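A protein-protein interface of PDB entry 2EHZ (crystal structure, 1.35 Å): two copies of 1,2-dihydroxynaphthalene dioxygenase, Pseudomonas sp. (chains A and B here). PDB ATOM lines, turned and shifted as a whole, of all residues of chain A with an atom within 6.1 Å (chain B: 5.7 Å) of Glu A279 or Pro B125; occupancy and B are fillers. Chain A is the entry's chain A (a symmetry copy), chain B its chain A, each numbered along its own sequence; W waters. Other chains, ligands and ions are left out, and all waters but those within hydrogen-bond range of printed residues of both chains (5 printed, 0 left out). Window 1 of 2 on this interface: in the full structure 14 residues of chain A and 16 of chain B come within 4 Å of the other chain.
NH2 of Arg B71 sits at hydrogen-bond distance from O of Ala A278 (2.9 Å).
The side-chain hydroxyl of Tyr A280 lies within hydrogen-bond range of the backbone carbonyl oxygen of Met B104.
The backbone carbonyl oxygen (O) of Pro B125 sits at hydrogen-bond distance from the backbone NH (N) of Tyr A280, 3.0 Å away.
The backbone NH (N) of Ile B127 lies within hydrogen-bond range of the backbone carbonyl oxygen (O) of Tyr A280 (2.9 Å).
The backbone NH (N) of Arg B126 is in hydrogen-bond range of the backbone carbonyl oxygen (O) of Met B104, at 3.3 Å.
The backbone NH (N) of Leu B106 is in hydrogen-bond range of the backbone carbonyl oxygen (O) of Gly B124, 3.1 Å away.
O of Glu A177 lies within hydrogen-bond range of N of Tyr A281, at 2.8 Å.
O of Ala A248 lies within hydrogen-bond range of NZ of Lys A251 (2.8 Å).
The side-chain amino group (NZ) of Lys A251 lies within hydrogen-bond range of the backbone carbonyl oxygen (O) of Asn A249, 3.0 Å away.
The side-chain carboxylate of Glu A279 lies within hydrogen-bond range of the side-chain hydroxyl of Tyr A281 (2.5 Å).
Among the printed residues, merely in contact across the chains: Ala A278 with Pro B125, Tyr A280 with Gly B124, Tyr A281 with Ile B127, Val A176 with Leu B106, Ala A278 with Gly B124, Tyr A280 with Arg B126, Glu A277 with Arg B71, Glu A279 with Pro B125, Glu A279 with Ile B127, Tyr A280 with Leu B106, Ala A278 with Trp B123, Lys A251 with Met B129, Tyr A281 with Met B129, Ala A248 with Met B129 and Glu A279 with Arg B71.
Printed residues of chain B within 4 Å of Glu A279: Arg B71 (3.98 Å), Pro B125 (3.6 Å) and Ile B127 (3.6 Å).
Of the printed residues of chain B, Tyr A280 touches Met B104, Leu B106, Gly B124, Pro B125, Arg B126 and Ile B127.
Of the printed residues of chain B, Tyr A281 touches Ile B127 and Met B129.
Of the printed residues of chain A, Arg B71 touches Glu A277 (3.6 Å), Ala A278 (2.9 Å) and Glu A279 (3.98 Å).
Of the printed residues of chain A, Met B129 touches Ala A248, Lys A251 and Tyr A281.
The nearest residue of chain A that does not touch Pro B125 is Tyr A281 (5.5 Å).
The nearest printed residue of chain A that does not touch Trp B123 is Val A176 (4.8 Å).
Hydrophobic or aromatic side chains of chain A that line the printed part of chain B: Ala A248, Ala A278, Tyr A280 and Tyr A281.
Along chain A the printed residues that touch a printed residue of chain B span positions 176 to 281.
Hydrophobic or aromatic side chains of chain B within 4 Å of the printed part of chain A: Met B104, Leu B106, Trp B123, Pro B125, Ile B127 and Met B129.
Among the printed residues, no Asp or Glu carboxylate lies within 4 Å of a Lys or Arg side-chain nitrogen of the other chain.
No position is printed for both chains.
Of the 19 pairs that touch across the chains among the printed residues, none has its exchanged pair printed and touching as well.
Water W4 lies within hydrogen-bond range of the side-chain carboxylate of Glu A279 (2.8 Å), the side-chain amino group of Lys A251 (2.8 Å) and the side-chain sulfur of Met B129 (3.5 Å).
Water W1 lies within hydrogen-bond range of the backbone carbonyl oxygen (O) of Ala A278, the guanidinium group (NE) of Arg B71 and the backbone NH (N) of Gly B124.
Water W3 lies within hydrogen-bond range of the side-chain carboxylate (OE2) of Glu A279 (2.8 Å) and the guanidinium group (NH2) of Arg B71 (3.0 Å).
Water W2 lies within hydrogen-bond range of O of Val B105 (2.9 Å) and OH of Tyr A280 (2.9 Å).
Water W5 lies within hydrogen-bond range of OH of Tyr A280 and NH1 of Arg B126.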
ATOM      1  N   VAL A 176     -18.741 -33.260  -9.607  1.00  0.00           N
ATOM      2  CA  VAL A 176     -19.579 -32.777 -10.698  1.00  0.00           C
ATOM      3  C   VAL A 176     -18.837 -31.683 -11.463  1.00  0.00           C
ATOM      4  O   VAL A 176     -18.449 -30.668 -10.878  1.00  0.00           O
ATOM      5  CB  VAL A 176     -20.913 -32.224 -10.159  1.00  0.00           C
ATOM      6  CG1 VAL A 176     -21.712 -31.558 -11.275  1.00  0.00           C
ATOM      7  CG2 VAL A 176     -21.728 -33.345  -9.507  1.00  0.00           C
ATOM      8  N   GLU A 177     -18.630 -31.894 -12.764  1.00  0.00           N
ATOM      9  CA  GLU A 177     -17.991 -30.879 -13.615  1.00  0.00           C
ATOM     10  C   GLU A 177     -18.927 -30.333 -14.679  1.00  0.00           C
ATOM     11  O   GLU A 177     -18.630 -29.310 -15.285  1.00  0.00           O
ATOM     12  CB  GLU A 177     -16.687 -31.391 -14.257  1.00  0.00           C
ATOM     13  CG  GLU A 177     -15.574 -31.598 -13.242  1.00  0.00           C
ATOM     14  CD  GLU A 177     -14.290 -32.150 -13.825  1.00  0.00           C
ATOM     15  OE1 GLU A 177     -14.246 -32.460 -15.038  1.00  0.00           O
ATOM     16  OE2 GLU A 177     -13.315 -32.284 -13.052  1.00  0.00           O
ATOM     17  N   TYR A 178     -20.044 -31.016 -14.931  1.00  0.00           N
ATOM     18  CA  TYR A 178     -21.020 -30.519 -15.892  1.00  0.00           C
ATOM     19  C   TYR A 178     -22.414 -30.571 -15.331  1.00  0.00           C
ATOM     20  O   TYR A 178     -22.821 -31.573 -14.738  1.00  0.00           O
ATOM     21  CB  TYR A 178     -21.009 -31.347 -17.167  1.00  0.00           C
ATOM     22  CG  TYR A 178     -19.785 -31.138 -18.022  1.00  0.00           C
ATOM     23  CD1 TYR A 178     -18.577 -31.747 -17.696  1.00  0.00           C
ATOM     24  CD2 TYR A 178     -19.838 -30.345 -19.163  1.00  0.00           C
ATOM     25  CE1 TYR A 178     -17.439 -31.572 -18.489  1.00  0.00           C
ATOM     26  CE2 TYR A 178     -18.702 -30.165 -19.969  1.00  0.00           C
ATOM     27  CZ  TYR A 178     -17.522 -30.780 -19.621  1.00  0.00           C
ATOM     28  OH  TYR A 178     -16.407 -30.619 -20.415  1.00  0.00           O
ATOM     29  N   ALA A 248     -14.843 -28.789 -22.390  1.00  0.00           N
ATOM     30  CA  ALA A 248     -14.468 -27.722 -21.456  1.00  0.00           C
ATOM     31  C   ALA A 248     -13.508 -28.184 -20.356  1.00  0.00           C
ATOM     32  O   ALA A 248     -12.632 -27.422 -19.959  1.00  0.00           O
ATOM     33  CB  ALA A 248     -15.708 -27.065 -20.861  1.00  0.00           C
ATOM     34  N   ASN A 249     -13.658 -29.416 -19.864  1.00  0.00           N
ATOM     35  CA  ASN A 249     -12.750 -29.884 -18.813  1.00  0.00           C
ATOM     36  C   ASN A 249     -11.338 -30.213 -19.289  1.00  0.00           C
ATOM     37  O   ASN A 249     -10.379 -29.607 -18.818  1.00  0.00           O
ATOM     38  CB  ASN A 249     -13.354 -31.001 -17.915  1.00  0.00           C
ATOM     39  CG  ASN A 249     -13.772 -32.267 -18.672  1.00  0.00           C
ATOM     40  OD1 ASN A 249     -13.567 -32.419 -19.882  1.00  0.00           O
ATOM     41  ND2 ASN A 249     -14.367 -33.201 -17.931  1.00  0.00           N
ATOM     42  N   LYS A 251     -10.089 -30.042 -22.510  1.00  0.00           N
ATOM     43  CA  LYS A 251      -9.630 -29.291 -23.686  1.00  0.00           C
ATOM     44  C   LYS A 251      -9.277 -30.198 -24.882  1.00  0.00           C
ATOM     45  O   LYS A 251      -8.635 -29.745 -25.817  1.00  0.00           O
ATOM     46  CB  LYS A 251      -8.440 -28.371 -23.340  1.00  0.00           C
ATOM     47  CG  LYS A 251      -8.532 -27.622 -21.993  1.00  0.00           C
ATOM     48  CD  LYS A 251      -9.721 -26.666 -21.939  1.00  0.00           C
ATOM     49  CE  LYS A 251      -9.769 -25.854 -20.639  1.00  0.00           C
ATOM     50  NZ  LYS A 251      -9.999 -26.708 -19.420  1.00  0.00           N
ATOM     51  N   ILE A 275      -6.630 -31.210 -13.069  1.00  0.00           N
ATOM     52  CA  ILE A 275      -6.477 -30.233 -11.986  1.00  0.00           C
ATOM     53  C   ILE A 275      -7.221 -30.675 -10.733  1.00  0.00           C
ATOM     54  O   ILE A 275      -8.303 -31.240 -10.842  1.00  0.00           O
ATOM     55  CB  ILE A 275      -6.887 -28.795 -12.409  1.00  0.00           C
ATOM     56  CG1 ILE A 275      -8.344 -28.723 -12.879  1.00  0.00           C
ATOM     57  CG2 ILE A 275      -5.938 -28.255 -13.486  1.00  0.00           C
ATOM     58  CD1 ILE A 275      -8.843 -27.287 -13.011  1.00  0.00           C
ATOM     59  N   GLU A 277      -8.342 -28.611  -8.454  1.00  0.00           N
ATOM     60  CA  GLU A 277      -9.327 -27.575  -8.124  1.00  0.00           C
ATOM     61  C   GLU A 277     -10.616 -27.765  -8.929  1.00  0.00           C
ATOM     62  O   GLU A 277     -10.616 -27.657 -10.160  1.00  0.00           O
ATOM     63  CB  GLU A 277      -8.733 -26.181  -8.360  1.00  0.00           C
ATOM     64  CG  GLU A 277      -7.435 -25.884  -7.575  1.00  0.00           C
ATOM     65  CD  GLU A 277      -6.199 -26.583  -8.134  1.00  0.00           C
ATOM     66  OE1 GLU A 277      -6.118 -26.796  -9.365  1.00  0.00           O
ATOM     67  OE2 GLU A 277      -5.300 -26.924  -7.333  1.00  0.00           O
ATOM     68  N   ALA A 278     -11.706 -28.058  -8.229  1.00  0.00           N
ATOM     69  CA  ALA A 278     -12.990 -28.347  -8.851  1.00  0.00           C
ATOM     70  C   ALA A 278     -13.593 -27.113  -9.509  1.00  0.00           C
ATOM     71  O   ALA A 278     -13.706 -26.053  -8.880  1.00  0.00           O
ATOM     72  CB  ALA A 278     -13.956 -28.900  -7.805  1.00  0.00           C
ATOM     73  N   GLU A 279     -14.006 -27.258 -10.763  1.00  0.00           N
ATOM     74  CA  GLU A 279     -14.829 -26.246 -11.416  1.00  0.00           C
ATOM     75  C   GLU A 279     -15.932 -26.949 -12.199  1.00  0.00           C
ATOM     76  O   GLU A 279     -15.902 -28.177 -12.349  1.00  0.00           O
ATOM     77  CB  GLU A 279     -13.992 -25.293 -12.271  1.00  0.00           C
ATOM     78  CG  GLU A 279     -13.262 -25.970 -13.398  1.00  0.00           C
ATOM     79  CD  GLU A 279     -12.182 -25.107 -14.095  1.00  0.00           C
ATOM     80  OE1 GLU A 279     -12.093 -25.199 -15.323  1.00  0.00           O
ATOM     81  OE2 GLU A 279     -11.412 -24.370 -13.450  1.00  0.00           O
ATOM     82  N   TYR A 280     -16.939 -26.196 -12.639  1.00  0.00           N
ATOM     83  CA  TYR A 280     -17.988 -26.786 -13.478  1.00  0.00           C
ATOM     84  C   TYR A 280     -18.382 -25.903 -14.649  1.00  0.00           C
ATOM     85  O   TYR A 280     -18.101 -24.698 -14.670  1.00  0.00           O
ATOM     86  CB  TYR A 280     -19.226 -27.207 -12.659  1.00  0.00           C
ATOM     87  CG  TYR A 280     -20.227 -26.110 -12.356  1.00  0.00           C
ATOM     88  CD1 TYR A 280     -20.025 -25.242 -11.283  1.00  0.00           C
ATOM     89  CD2 TYR A 280     -21.380 -25.950 -13.131  1.00  0.00           C
ATOM     90  CE1 TYR A 280     -20.953 -24.238 -10.985  1.00  0.00           C
ATOM     91  CE2 TYR A 280     -22.312 -24.946 -12.844  1.00  0.00           C
ATOM     92  CZ  TYR A 280     -22.093 -24.094 -11.769  1.00  0.00           C
ATOM     93  OH  TYR A 280     -23.008 -23.099 -11.477  1.00  0.00           O
ATOM     94  N   TYR A 281     -19.042 -26.544 -15.612  1.00  0.00           N
ATOM     95  CA  TYR A 281     -19.448 -25.921 -16.860  1.00  0.00           C
ATOM     96  C   TYR A 281     -20.879 -26.307 -17.160  1.00  0.00           C
ATOM     97  O   TYR A 281     -21.384 -27.301 -16.640  1.00  0.00           O
ATOM     98  CB  TYR A 281     -18.551 -26.401 -18.019  1.00  0.00           C
ATOM     99  CG  TYR A 281     -17.115 -26.616 -17.601  1.00  0.00           C
ATOM    100  CD1 TYR A 281     -16.672 -27.879 -17.212  1.00  0.00           C
ATOM    101  CD2 TYR A 281     -16.210 -25.558 -17.568  1.00  0.00           C
ATOM    102  CE1 TYR A 281     -15.365 -28.084 -16.792  1.00  0.00           C
ATOM    103  CE2 TYR A 281     -14.896 -25.759 -17.154  1.00  0.00           C
ATOM    104  CZ  TYR A 281     -14.483 -27.026 -16.773  1.00  0.00           C
ATOM    105  OH  TYR A 281     -13.192 -27.235 -16.347  1.00  0.00           O
ATOM    106  N   TRP B  51     -14.199 -17.263 -16.275  1.00  0.00           N
ATOM    107  CA  TRP B  51     -15.240 -17.450 -15.258  1.00  0.00           C
ATOM    108  C   TRP B  51     -16.535 -16.797 -15.724  1.00  0.00           C
ATOM    109  O   TRP B  51     -16.500 -15.773 -16.425  1.00  0.00           O
ATOM    110  CB  TRP B  51     -14.810 -16.849 -13.925  1.00  0.00           C
ATOM    111  CG  TRP B  51     -13.798 -17.685 -13.173  1.00  0.00           C
ATOM    112  CD1 TRP B  51     -12.724 -18.379 -13.690  1.00  0.00           C
ATOM    113  CD2 TRP B  51     -13.771 -17.902 -11.758  1.00  0.00           C
ATOM    114  NE1 TRP B  51     -12.046 -19.018 -12.673  1.00  0.00           N
ATOM    115  CE2 TRP B  51     -12.669 -18.743 -11.482  1.00  0.00           C
ATOM    116  CE3 TRP B  51     -14.583 -17.478 -10.695  1.00  0.00           C
ATOM    117  CZ2 TRP B  51     -12.352 -19.160 -10.182  1.00  0.00           C
ATOM    118  CZ3 TRP B  51     -14.261 -17.887  -9.405  1.00  0.00           C
ATOM    119  CH2 TRP B  51     -13.163 -18.726  -9.165  1.00  0.00           C
ATOM    120  N   ARG B  71     -12.484 -19.175  -2.536  1.00  0.00           N
ATOM    121  CA  ARG B  71     -12.564 -20.520  -3.090  1.00  0.00           C
ATOM    122  C   ARG B  71     -11.692 -21.506  -2.317  1.00  0.00           C
ATOM    123  O   ARG B  71     -10.599 -21.154  -1.865  1.00  0.00           O
ATOM    124  CB  ARG B  71     -12.095 -20.477  -4.545  1.00  0.00           C
ATOM    125  CG  ARG B  71     -12.246 -21.771  -5.330  1.00  0.00           C
ATOM    126  CD  ARG B  71     -11.589 -21.639  -6.694  1.00  0.00           C
ATOM    127  NE  ARG B  71     -11.832 -22.825  -7.507  1.00  0.00           N
ATOM    128  CZ  ARG B  71     -11.245 -23.058  -8.674  1.00  0.00           C
ATOM    129  NH1 ARG B  71     -10.359 -22.196  -9.170  1.00  0.00           N
ATOM    130  NH2 ARG B  71     -11.541 -24.166  -9.349  1.00  0.00           N
ATOM    131  N   MET B 104     -23.795 -19.249  -8.309  1.00  0.00           N
ATOM    132  CA  MET B 104     -23.295 -20.136  -9.373  1.00  0.00           C
ATOM    133  C   MET B 104     -22.076 -20.941  -8.920  1.00  0.00           C
ATOM    134  O   MET B 104     -21.038 -20.992  -9.594  1.00  0.00           O
ATOM    135  CB  MET B 104     -23.037 -19.360 -10.668  1.00  0.00           C
ATOM    136  CG  MET B 104     -24.302 -18.715 -11.192  1.00  0.00           C
ATOM    137  SD  MET B 104     -23.966 -17.597 -12.548  1.00  0.00           S
ATOM    138  CE  MET B 104     -25.224 -16.359 -12.264  1.00  0.00           C
ATOM    139  N   VAL B 105     -22.229 -21.583  -7.767  1.00  0.00           N
ATOM    140  CA  VAL B 105     -21.183 -22.426  -7.198  1.00  0.00           C
ATOM    141  C   VAL B 105     -21.788 -23.764  -6.785  1.00  0.00           C
ATOM    142  O   VAL B 105     -23.015 -23.879  -6.612  1.00  0.00           O
ATOM    143  CB  VAL B 105     -20.482 -21.753  -5.984  1.00  0.00           C
ATOM    144  CG1 VAL B 105     -19.860 -20.416  -6.392  1.00  0.00           C
ATOM    145  CG2 VAL B 105     -21.453 -21.556  -4.822  1.00  0.00           C
ATOM    146  N   LEU B 106     -20.936 -24.770  -6.614  1.00  0.00           N
ATOM    147  CA  LEU B 106     -21.434 -26.103  -6.236  1.00  0.00           C
ATOM    148  C   LEU B 106     -21.683 -26.278  -4.742  1.00  0.00           C
ATOM    149  O   LEU B 106     -22.555 -27.051  -4.349  1.00  0.00           O
ATOM    150  CB  LEU B 106     -20.529 -27.211  -6.772  1.00  0.00           C
ATOM    151  CG  LEU B 106     -20.442 -27.255  -8.301  1.00  0.00           C
ATOM    152  CD1 LEU B 106     -19.450 -28.311  -8.724  1.00  0.00           C
ATOM    153  CD2 LEU B 106     -21.802 -27.485  -8.962  1.00  0.00           C
ATOM    154  N   PHE B 122     -16.566 -21.147  -0.754  1.00  0.00           N
ATOM    155  CA  PHE B 122     -17.232 -21.973  -1.756  1.00  0.00           C
ATOM    156  C   PHE B 122     -16.273 -22.917  -2.444  1.00  0.00           C
ATOM    157  O   PHE B 122     -15.057 -22.717  -2.418  1.00  0.00           O
ATOM    158  CB  PHE B 122     -17.927 -21.092  -2.808  1.00  0.00           C
ATOM    159  CG  PHE B 122     -16.985 -20.453  -3.798  1.00  0.00           C
ATOM    160  CD1 PHE B 122     -16.740 -21.057  -5.029  1.00  0.00           C
ATOM    161  CD2 PHE B 122     -16.334 -19.259  -3.499  1.00  0.00           C
ATOM    162  CE1 PHE B 122     -15.879 -20.485  -5.949  1.00  0.00           C
ATOM    163  CE2 PHE B 122     -15.459 -18.678  -4.422  1.00  0.00           C
ATOM    164  CZ  PHE B 122     -15.240 -19.296  -5.652  1.00  0.00           C
ATOM    165  N   TRP B 123     -16.841 -23.937  -3.081  1.00  0.00           N
ATOM    166  CA  TRP B 123     -16.101 -24.732  -4.049  1.00  0.00           C
ATOM    167  C   TRP B 123     -16.902 -24.836  -5.339  1.00  0.00           C
ATOM    168  O   TRP B 123     -18.132 -24.742  -5.328  1.00  0.00           O
ATOM    169  CB  TRP B 123     -15.747 -26.126  -3.501  1.00  0.00           C
ATOM    170  CG  TRP B 123     -16.904 -27.082  -3.385  1.00  0.00           C
ATOM    171  CD1 TRP B 123     -17.774 -27.201  -2.338  1.00  0.00           C
ATOM    172  CD2 TRP B 123     -17.295 -28.065  -4.347  1.00  0.00           C
ATOM    173  NE1 TRP B 123     -18.690 -28.196  -2.595  1.00  0.00           N
ATOM    174  CE2 TRP B 123     -18.419 -28.742  -3.822  1.00  0.00           C
ATOM    175  CE3 TRP B 123     -16.809 -28.437  -5.604  1.00  0.00           C
ATOM    176  CZ2 TRP B 123     -19.071 -29.770  -4.515  1.00  0.00           C
ATOM    177  CZ3 TRP B 123     -17.453 -29.470  -6.292  1.00  0.00           C
ATOM    178  CH2 TRP B 123     -18.575 -30.120  -5.742  1.00  0.00           C
ATOM    179  N   GLY B 124     -16.198 -25.023  -6.448  1.00  0.00           N
ATOM    180  CA  GLY B 124     -16.849 -25.269  -7.728  1.00  0.00           C
ATOM    181  C   GLY B 124     -17.443 -24.050  -8.403  1.00  0.00           C
ATOM    182  O   GLY B 124     -18.664 -23.968  -8.560  1.00  0.00           O
ATOM    183  N   PRO B 125     -16.585 -23.112  -8.841  1.00  0.00           N
ATOM    184  CA  PRO B 125     -17.064 -21.976  -9.621  1.00  0.00           C
ATOM    185  C   PRO B 125     -17.547 -22.425 -10.998  1.00  0.00           C
ATOM    186  O   PRO B 125     -17.099 -23.458 -11.517  1.00  0.00           O
ATOM    187  CB  PRO B 125     -15.811 -21.113  -9.789  1.00  0.00           C
ATOM    188  CG  PRO B 125     -14.687 -22.090  -9.738  1.00  0.00           C
ATOM    189  CD  PRO B 125     -15.117 -23.082  -8.690  1.00  0.00           C
ATOM    190  N   ARG B 126     -18.443 -21.635 -11.576  1.00  0.00           N
ATOM    191  CA  ARG B 126     -18.910 -21.831 -12.927  1.00  0.00           C
ATOM    192  C   ARG B 126     -17.963 -21.143 -13.897  1.00  0.00           C
ATOM    193  O   ARG B 126     -17.707 -19.939 -13.789  1.00  0.00           O
ATOM    194  CB  ARG B 126     -20.313 -21.262 -13.102  1.00  0.00           C
ATOM    195  CG  ARG B 126     -20.813 -21.434 -14.522  1.00  0.00           C
ATOM    196  CD  ARG B 126     -22.181 -20.857 -14.724  1.00  0.00           C
ATOM    197  NE  ARG B 126     -22.381 -20.522 -16.131  1.00  0.00           N
ATOM    198  CZ  ARG B 126     -23.563 -20.271 -16.685  1.00  0.00           C
ATOM    199  NH1 ARG B 126     -24.673 -20.353 -15.964  1.00  0.00           N
ATOM    200  NH2 ARG B 126     -23.636 -19.954 -17.969  1.00  0.00           N
ATOM    201  N   ILE B 127     -17.453 -21.920 -14.850  1.00  0.00           N
ATOM    202  CA  ILE B 127     -16.532 -21.431 -15.862  1.00  0.00           C
ATOM    203  C   ILE B 127     -17.227 -21.546 -17.210  1.00  0.00           C
ATOM    204  O   ILE B 127     -17.732 -22.618 -17.561  1.00  0.00           O
ATOM    205  CB  ILE B 127     -15.230 -22.267 -15.887  1.00  0.00           C
ATOM    206  CG1 ILE B 127     -14.661 -22.510 -14.477  1.00  0.00           C
ATOM    207  CG2 ILE B 127     -14.202 -21.659 -16.847  1.00  0.00           C
ATOM    208  CD1 ILE B 127     -14.420 -21.289 -13.629  1.00  0.00           C
ATOM    209  N   MET B 129     -16.209 -21.720 -20.550  1.00  0.00           N
ATOM    210  CA  MET B 129     -15.147 -21.936 -21.537  1.00  0.00           C
ATOM    211  C   MET B 129     -15.597 -21.592 -22.951  1.00  0.00           C
ATOM    212  O   MET B 129     -14.773 -21.236 -23.798  1.00  0.00           O
ATOM    213  CB  MET B 129     -14.637 -23.382 -21.501  1.00  0.00           C
ATOM    214  CG  MET B 129     -13.827 -23.740 -20.257  1.00  0.00           C
ATOM    215  SD  MET B 129     -12.478 -22.581 -19.872  1.00  0.00           S
ATOM    216  CE  MET B 129     -11.509 -22.570 -21.382  1.00  0.00           C
HETATM  217  O   HOH W   1     -13.290 -25.032  -6.322  1.00  0.00           O
HETATM  218  O   HOH W   2     -24.582 -23.650  -9.071  1.00  0.00           O
HETATM  219  O   HOH W   3      -9.459 -23.921 -11.447  1.00  0.00           O
HETATM  220  O   HOH W   4     -10.693 -24.651 -17.630  1.00  0.00           O
HETATM  221  O   HOH W   5     -25.256 -22.285 -13.226  1.00  0.00           O
